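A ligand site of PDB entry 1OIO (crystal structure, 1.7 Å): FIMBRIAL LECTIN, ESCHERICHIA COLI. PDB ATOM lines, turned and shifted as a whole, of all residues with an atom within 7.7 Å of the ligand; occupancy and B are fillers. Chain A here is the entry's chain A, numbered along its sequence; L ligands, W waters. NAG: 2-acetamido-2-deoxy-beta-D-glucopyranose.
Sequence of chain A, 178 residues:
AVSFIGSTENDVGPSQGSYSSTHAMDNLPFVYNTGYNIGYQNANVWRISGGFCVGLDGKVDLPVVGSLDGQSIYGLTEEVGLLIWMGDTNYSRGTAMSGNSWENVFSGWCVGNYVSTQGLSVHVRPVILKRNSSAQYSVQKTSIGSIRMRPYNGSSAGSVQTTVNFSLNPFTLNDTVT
An oxygen (O3) of the ligand lies within hydrogen-bond range of the side-chain hydroxyl (OG1) of Thr 89.
An oxygen (O6) of the ligand is in hydrogen-bond range of the side-chain carboxylate (OD2) of Asp 88.
O of Ala 43 sits at hydrogen-bond distance from O3 of the ligand, 2.7 Å away.
The backbone NH of Gly 119 is in hydrogen-bond range of an oxygen (O4) of the ligand (2.8 Å).
A nitrogen (N2) of the ligand is in hydrogen-bond range of the side-chain hydroxyl (OG1) of Thr 117 (2.9 Å).
O4 of the ligand sits at hydrogen-bond distance from NE2 of Gln 118 (3.2 Å).
OD1 of Asp 88 sits at hydrogen-bond distance from NE2 of Gln 118.
The side-chain carboxylate of Asp 88 lies within salt-bridge range of the guanidinium group of Arg 93, 3.0 Å away.
The backbone NH of Gly 119 lies within hydrogen-bond range of the backbone carbonyl oxygen of Ala 43, at 3.5 Å.
O of Ala 43 is in hydrogen-bond range of OG1 of Thr 117, at 3.1 Å.
OG1 of Thr 117 lies within hydrogen-bond range of OD1 of Asn 44, 2.9 Å away.
OE1 of Gln 118 is in hydrogen-bond range of NE1 of Trp 109 (2.8 Å).
The backbone NH (N) of Val 45 sits at hydrogen-bond distance from the backbone carbonyl oxygen (O) of Gln 118, 3.0 Å away.
The backbone NH (N) of Ser 116 is in hydrogen-bond range of the backbone carbonyl oxygen (O) of Ile 48.
OD1 of Asn 44 touches C8 of the ligand, at 3.3 Å.
Arg 93 touches the ligand.
Trp 109 touches the ligand.
Ser 116 touches the ligand.
Hydrophobic or aromatic side chains that line the ligand: Ala 43 and Trp 109.
Of the 22 residues printed, 10 come within 4 Å of the ligand.
The nearest printed residue that does not touch the ligand is Phe 106 (4.1 Å).
Water W3 bridges O1 of the ligand (2.7 Å) and OG of Ser 116 (2.7 Å).
Water W2 bridges OG of Ser 116 (2.9 Å) and N2 of the ligand (3.4 Å).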
ATOM      1  N   ASN A  42      32.845  26.693  -1.275  1.00  0.00           N
ATOM      2  CA  ASN A  42      32.016  26.251  -0.164  1.00  0.00           C
ATOM      3  C   ASN A  42      30.667  25.846  -0.753  1.00  0.00           C
ATOM      4  O   ASN A  42      29.965  26.657  -1.329  1.00  0.00           O
ATOM      5  CB  ASN A  42      31.812  27.372   0.862  1.00  0.00           C
ATOM      6  CG  ASN A  42      31.203  26.869   2.152  1.00  0.00           C
ATOM      7  OD1 ASN A  42      30.397  25.933   2.155  1.00  0.00           O
ATOM      8  ND2 ASN A  42      31.564  27.488   3.269  1.00  0.00           N
ATOM      9  N   ALA A  43      30.333  24.572  -0.602  1.00  0.00           N
ATOM     10  CA  ALA A  43      29.071  24.070  -1.130  1.00  0.00           C
ATOM     11  C   ALA A  43      27.881  24.511  -0.285  1.00  0.00           C
ATOM     12  O   ALA A  43      26.735  24.407  -0.715  1.00  0.00           O
ATOM     13  CB  ALA A  43      29.105  22.557  -1.215  1.00  0.00           C
ATOM     14  N   ASN A  44      28.166  25.035   0.901  1.00  0.00           N
ATOM     15  CA  ASN A  44      27.105  25.431   1.817  1.00  0.00           C
ATOM     16  C   ASN A  44      27.193  26.852   2.345  1.00  0.00           C
ATOM     17  O   ASN A  44      27.746  27.091   3.423  1.00  0.00           O
ATOM     18  CB  ASN A  44      27.101  24.440   2.978  1.00  0.00           C
ATOM     19  CG  ASN A  44      27.127  22.998   2.508  1.00  0.00           C
ATOM     20  OD1 ASN A  44      26.152  22.486   1.959  1.00  0.00           O
ATOM     21  ND2 ASN A  44      28.278  22.335   2.685  1.00  0.00           N
ATOM     22  N   VAL A  45      26.625  27.802   1.600  1.00  0.00           N
ATOM     23  CA  VAL A  45      26.644  29.192   2.016  1.00  0.00           C
ATOM     24  C   VAL A  45      25.244  29.651   2.425  1.00  0.00           C
ATOM     25  O   VAL A  45      25.096  30.460   3.339  1.00  0.00           O
ATOM     26  CB  VAL A  45      27.199  30.090   0.894  1.00  0.00           C
ATOM     27  CG1 VAL A  45      27.266  31.534   1.360  1.00  0.00           C
ATOM     28  CG2 VAL A  45      28.590  29.603   0.516  1.00  0.00           C
ATOM     29  N   TRP A  46      24.232  29.112   1.744  1.00  0.00           N
ATOM     30  CA  TRP A  46      22.847  29.412   2.071  1.00  0.00           C
ATOM     31  C   TRP A  46      22.081  28.091   2.116  1.00  0.00           C
ATOM     32  O   TRP A  46      22.377  27.164   1.358  1.00  0.00           O
ATOM     33  CB  TRP A  46      22.177  30.301   1.012  1.00  0.00           C
ATOM     34  CG  TRP A  46      22.679  31.686   0.967  1.00  0.00           C
ATOM     35  CD1 TRP A  46      22.296  32.744   1.753  1.00  0.00           C
ATOM     36  CD2 TRP A  46      23.705  32.178   0.096  1.00  0.00           C
ATOM     37  NE1 TRP A  46      23.029  33.858   1.435  1.00  0.00           N
ATOM     38  CE2 TRP A  46      23.899  33.540   0.423  1.00  0.00           C
ATOM     39  CE3 TRP A  46      24.481  31.604  -0.910  1.00  0.00           C
ATOM     40  CZ2 TRP A  46      24.847  34.331  -0.236  1.00  0.00           C
ATOM     41  CZ3 TRP A  46      25.417  32.387  -1.570  1.00  0.00           C
ATOM     42  CH2 TRP A  46      25.598  33.741  -1.223  1.00  0.00           C
ATOM     43  N   ILE A  48      18.453  26.515   1.547  1.00  0.00           N
ATOM     44  CA  ILE A  48      17.225  26.869   0.859  1.00  0.00           C
ATOM     45  C   ILE A  48      16.212  25.720   0.860  1.00  0.00           C
ATOM     46  O   ILE A  48      16.586  24.542   0.961  1.00  0.00           O
ATOM     47  CB  ILE A  48      17.497  27.313  -0.600  1.00  0.00           C
ATOM     48  CG1 ILE A  48      18.231  26.223  -1.372  1.00  0.00           C
ATOM     49  CG2 ILE A  48      18.347  28.567  -0.586  1.00  0.00           C
ATOM     50  CD1 ILE A  48      18.369  26.562  -2.844  1.00  0.00           C
ATOM     51  N   VAL A  54      17.125  30.431  -6.524  1.00  0.00           N
ATOM     52  CA  VAL A  54      18.252  31.319  -6.294  1.00  0.00           C
ATOM     53  C   VAL A  54      19.416  31.155  -7.264  1.00  0.00           C
ATOM     54  O   VAL A  54      19.734  30.052  -7.692  1.00  0.00           O
ATOM     55  CB  VAL A  54      18.773  31.139  -4.857  1.00  0.00           C
ATOM     56  CG1 VAL A  54      19.411  29.764  -4.709  1.00  0.00           C
ATOM     57  CG2 VAL A  54      19.772  32.241  -4.515  1.00  0.00           C
ATOM     58  N   LEU A  56      23.359  33.460  -8.496  1.00  0.00           N
ATOM     59  CA  LEU A  56      24.451  34.216  -7.881  1.00  0.00           C
ATOM     60  C   LEU A  56      24.954  35.347  -8.766  1.00  0.00           C
ATOM     61  O   LEU A  56      25.081  35.176  -9.974  1.00  0.00           O
ATOM     62  CB  LEU A  56      25.644  33.303  -7.589  1.00  0.00           C
ATOM     63  CG  LEU A  56      25.519  32.062  -6.714  1.00  0.00           C
ATOM     64  CD1 LEU A  56      26.842  31.304  -6.783  1.00  0.00           C
ATOM     65  CD2 LEU A  56      25.191  32.437  -5.269  1.00  0.00           C
ATOM     66  N   GLY A  87      31.336  31.886  -9.300  1.00  0.00           N
ATOM     67  CA  GLY A  87      30.182  31.099  -9.728  1.00  0.00           C
ATOM     68  C   GLY A  87      29.688  30.113  -8.698  1.00  0.00           C
ATOM     69  O   GLY A  87      29.949  30.275  -7.495  1.00  0.00           O
ATOM     70  N   ASP A  88      28.983  29.099  -9.166  1.00  0.00           N
ATOM     71  CA  ASP A  88      28.439  28.057  -8.308  1.00  0.00           C
ATOM     72  C   ASP A  88      29.594  27.287  -7.664  1.00  0.00           C
ATOM     73  O   ASP A  88      30.760  27.514  -7.991  1.00  0.00           O
ATOM     74  CB  ASP A  88      27.538  27.111  -9.132  1.00  0.00           C
ATOM     75  CG  ASP A  88      26.642  26.255  -8.255  1.00  0.00           C
ATOM     76  OD1 ASP A  88      26.274  26.708  -7.148  1.00  0.00           O
ATOM     77  OD2 ASP A  88      26.279  25.130  -8.686  1.00  0.00           O
ATOM     78  N   THR A  89      29.251  26.400  -6.740  1.00  0.00           N
ATOM     79  CA  THR A  89      30.234  25.629  -5.987  1.00  0.00           C
ATOM     80  C   THR A  89      31.407  25.031  -6.755  1.00  0.00           C
ATOM     81  O   THR A  89      32.570  25.242  -6.399  1.00  0.00           O
ATOM     82  CB  THR A  89      29.536  24.504  -5.215  1.00  0.00           C
ATOM     83  OG1 THR A  89      28.378  25.034  -4.553  1.00  0.00           O
ATOM     84  CG2 THR A  89      30.464  23.918  -4.173  1.00  0.00           C
ATOM     85  N   ASN A  90      31.123  24.267  -7.800  1.00  0.00           N
ATOM     86  CA  ASN A  90      32.211  23.656  -8.563  1.00  0.00           C
ATOM     87  C   ASN A  90      33.016  24.708  -9.324  1.00  0.00           C
ATOM     88  O   ASN A  90      32.457  25.504 -10.071  1.00  0.00           O
ATOM     89  CB  ASN A  90      31.670  22.610  -9.540  1.00  0.00           C
ATOM     90  CG  ASN A  90      31.329  21.294  -8.866  1.00  0.00           C
ATOM     91  OD1 ASN A  90      32.068  20.824  -7.993  1.00  0.00           O
ATOM     92  ND2 ASN A  90      30.221  20.682  -9.279  1.00  0.00           N
ATOM     93  N   ARG A  93      32.458  25.662 -12.808  1.00  0.00           N
ATOM     94  CA  ARG A  93      31.300  26.485 -13.123  1.00  0.00           C
ATOM     95  C   ARG A  93      31.593  27.973 -12.956  1.00  0.00           C
ATOM     96  O   ARG A  93      30.698  28.798 -13.094  1.00  0.00           O
ATOM     97  CB  ARG A  93      30.110  26.088 -12.268  1.00  0.00           C
ATOM     98  CG  ARG A  93      29.483  24.773 -12.695  1.00  0.00           C
ATOM     99  CD  ARG A  93      28.241  24.486 -11.919  1.00  0.00           C
ATOM    100  NE  ARG A  93      27.555  23.302 -12.437  1.00  0.00           N
ATOM    101  CZ  ARG A  93      26.329  22.946 -12.078  1.00  0.00           C
ATOM    102  NH1 ARG A  93      25.678  23.685 -11.192  1.00  0.00           N
ATOM    103  NH2 ARG A  93      25.768  21.869 -12.593  1.00  0.00           N
ATOM    104  N   PHE A 106      25.837  32.825 -11.908  1.00  0.00           N
ATOM    105  CA  PHE A 106      25.163  31.528 -11.798  1.00  0.00           C
ATOM    106  C   PHE A 106      23.687  31.763 -12.085  1.00  0.00           C
ATOM    107  O   PHE A 106      22.998  32.424 -11.319  1.00  0.00           O
ATOM    108  CB  PHE A 106      25.333  30.918 -10.403  1.00  0.00           C
ATOM    109  CG  PHE A 106      24.602  29.615 -10.216  1.00  0.00           C
ATOM    110  CD1 PHE A 106      24.547  28.681 -11.237  1.00  0.00           C
ATOM    111  CD2 PHE A 106      23.963  29.330  -9.019  1.00  0.00           C
ATOM    112  CE1 PHE A 106      23.867  27.469 -11.072  1.00  0.00           C
ATOM    113  CE2 PHE A 106      23.283  28.129  -8.844  1.00  0.00           C
ATOM    114  CZ  PHE A 106      23.239  27.193  -9.865  1.00  0.00           C
ATOM    115  N   GLY A 108      21.198  30.046 -11.710  1.00  0.00           N
ATOM    116  CA  GLY A 108      20.334  29.620 -10.622  1.00  0.00           C
ATOM    117  C   GLY A 108      19.558  28.324 -10.779  1.00  0.00           C
ATOM    118  O   GLY A 108      19.553  27.675 -11.821  1.00  0.00           O
ATOM    119  N   TRP A 109      18.896  27.938  -9.700  1.00  0.00           N
ATOM    120  CA  TRP A 109      18.088  26.736  -9.713  1.00  0.00           C
ATOM    121  C   TRP A 109      17.040  26.910  -8.636  1.00  0.00           C
ATOM    122  O   TRP A 109      17.160  27.804  -7.788  1.00  0.00           O
ATOM    123  CB  TRP A 109      18.937  25.497  -9.418  1.00  0.00           C
ATOM    124  CG  TRP A 109      19.436  25.402  -7.996  1.00  0.00           C
ATOM    125  CD1 TRP A 109      20.300  26.246  -7.370  1.00  0.00           C
ATOM    126  CD2 TRP A 109      19.087  24.394  -7.047  1.00  0.00           C
ATOM    127  NE1 TRP A 109      20.514  25.818  -6.071  1.00  0.00           N
ATOM    128  CE2 TRP A 109      19.783  24.680  -5.852  1.00  0.00           C
ATOM    129  CE3 TRP A 109      18.245  23.270  -7.087  1.00  0.00           C
ATOM    130  CZ2 TRP A 109      19.670  23.895  -4.708  1.00  0.00           C
ATOM    131  CZ3 TRP A 109      18.139  22.474  -5.941  1.00  0.00           C
ATOM    132  CH2 TRP A 109      18.845  22.798  -4.768  1.00  0.00           C
ATOM    133  N   TYR A 114      11.753  20.388  -0.433  1.00  0.00           N
ATOM    134  CA  TYR A 114      12.773  19.776   0.405  1.00  0.00           C
ATOM    135  C   TYR A 114      13.842  20.813   0.735  1.00  0.00           C
ATOM    136  O   TYR A 114      13.811  21.925   0.227  1.00  0.00           O
ATOM    137  CB  TYR A 114      13.397  18.569  -0.298  1.00  0.00           C
ATOM    138  CG  TYR A 114      14.138  18.870  -1.589  1.00  0.00           C
ATOM    139  CD1 TYR A 114      15.523  19.032  -1.598  1.00  0.00           C
ATOM    140  CD2 TYR A 114      13.454  18.939  -2.801  1.00  0.00           C
ATOM    141  CE1 TYR A 114      16.219  19.254  -2.778  1.00  0.00           C
ATOM    142  CE2 TYR A 114      14.141  19.163  -3.991  1.00  0.00           C
ATOM    143  CZ  TYR A 114      15.522  19.316  -3.970  1.00  0.00           C
ATOM    144  OH  TYR A 114      16.213  19.509  -5.149  1.00  0.00           O
ATOM    145  N   SER A 116      17.874  21.991   0.827  1.00  0.00           N
ATOM    146  CA  SER A 116      19.168  21.781   0.188  1.00  0.00           C
ATOM    147  C   SER A 116      20.023  23.014   0.495  1.00  0.00           C
ATOM    148  O   SER A 116      19.712  23.775   1.411  1.00  0.00           O
ATOM    149  CB  SER A 116      19.007  21.598  -1.318  1.00  0.00           C
ATOM    150  OG  SER A 116      20.207  21.143  -1.911  1.00  0.00           O
ATOM    151  N   THR A 117      21.110  23.201  -0.247  1.00  0.00           N
ATOM    152  CA  THR A 117      21.955  24.362  -0.018  1.00  0.00           C
ATOM    153  C   THR A 117      22.426  24.985  -1.322  1.00  0.00           C
ATOM    154  O   THR A 117      22.329  24.375  -2.392  1.00  0.00           O
ATOM    155  CB  THR A 117      23.206  24.019   0.801  1.00  0.00           C
ATOM    156  OG1 THR A 117      24.008  23.080   0.076  1.00  0.00           O
ATOM    157  CG2 THR A 117      22.817  23.411   2.140  1.00  0.00           C
ATOM    158  N   GLN A 118      22.916  26.215  -1.220  1.00  0.00           N
ATOM    159  CA  GLN A 118      23.450  26.953  -2.365  1.00  0.00           C
ATOM    160  C   GLN A 118      24.870  27.336  -1.961  1.00  0.00           C
ATOM    161  O   GLN A 118      25.078  27.933  -0.913  1.00  0.00           O
ATOM    162  CB  GLN A 118      22.634  28.217  -2.630  1.00  0.00           C
ATOM    163  CG  GLN A 118      23.238  29.127  -3.699  1.00  0.00           C
ATOM    164  CD  GLN A 118      23.407  28.422  -5.028  1.00  0.00           C
ATOM    165  OE1 GLN A 118      22.503  27.734  -5.504  1.00  0.00           O
ATOM    166  NE2 GLN A 118      24.564  28.599  -5.644  1.00  0.00           N
ATOM    167  N   GLY A 119      25.836  26.993  -2.815  1.00  0.00           N
ATOM    168  CA  GLY A 119      27.221  27.318  -2.521  1.00  0.00           C
ATOM    169  C   GLY A 119      27.784  28.301  -3.516  1.00  0.00           C
ATOM    170  O   GLY A 119      27.045  28.981  -4.229  1.00  0.00           O
ATOM    171  N   LEU A 120      29.104  28.382  -3.565  1.00  0.00           N
ATOM    172  CA  LEU A 120      29.768  29.285  -4.489  1.00  0.00           C
ATOM    173  C   LEU A 120      31.241  28.955  -4.569  1.00  0.00           C
ATOM    174  O   LEU A 120      31.752  28.130  -3.804  1.00  0.00           O
ATOM    175  CB  LEU A 120      29.583  30.739  -4.040  1.00  0.00           C
ATOM    176  CG  LEU A 120      29.791  31.044  -2.557  1.00  0.00           C
ATOM    177  CD1 LEU A 120      31.251  30.867  -2.173  1.00  0.00           C
ATOM    178  CD2 LEU A 120      29.357  32.473  -2.273  1.00  0.00           C
HETATM  179  C1  NAG L   1      23.451  21.827  -4.273  1.00  0.00           C
HETATM  180  C2  NAG L   1      24.831  22.042  -3.663  1.00  0.00           C
HETATM  181  C3  NAG L   1      25.202  23.537  -3.701  1.00  0.00           C
HETATM  182  C4  NAG L   1      25.015  24.109  -5.106  1.00  0.00           C
HETATM  183  C5  NAG L   1      23.615  23.778  -5.641  1.00  0.00           C
HETATM  184  C6  NAG L   1      23.425  24.227  -7.070  1.00  0.00           C
HETATM  185  C7  NAG L   1      25.658  20.623  -1.905  1.00  0.00           C
HETATM  186  C8  NAG L   1      25.694  20.290  -0.422  1.00  0.00           C
HETATM  187  N2  NAG L   1      24.840  21.587  -2.286  1.00  0.00           N
HETATM  188  O1  NAG L   1      23.177  20.471  -4.335  1.00  0.00           O
HETATM  189  O3  NAG L   1      26.547  23.701  -3.302  1.00  0.00           O
HETATM  190  O4  NAG L   1      25.198  25.513  -5.062  1.00  0.00           O
HETATM  191  O5  NAG L   1      23.412  22.350  -5.605  1.00  0.00           O
HETATM  192  O6  NAG L   1      24.325  23.560  -7.943  1.00  0.00           O
HETATM  193  O7  NAG L   1      26.376  19.997  -2.691  1.00  0.00           O
HETATM  194  O   HOH W   1      28.374  20.761  -4.596  1.00  0.00           O
HETATM  195  O   HOH W   2      22.453  19.804  -0.577  1.00  0.00           O
HETATM  196  O   HOH W   3      20.539  20.039  -4.324  1.00  0.00           O
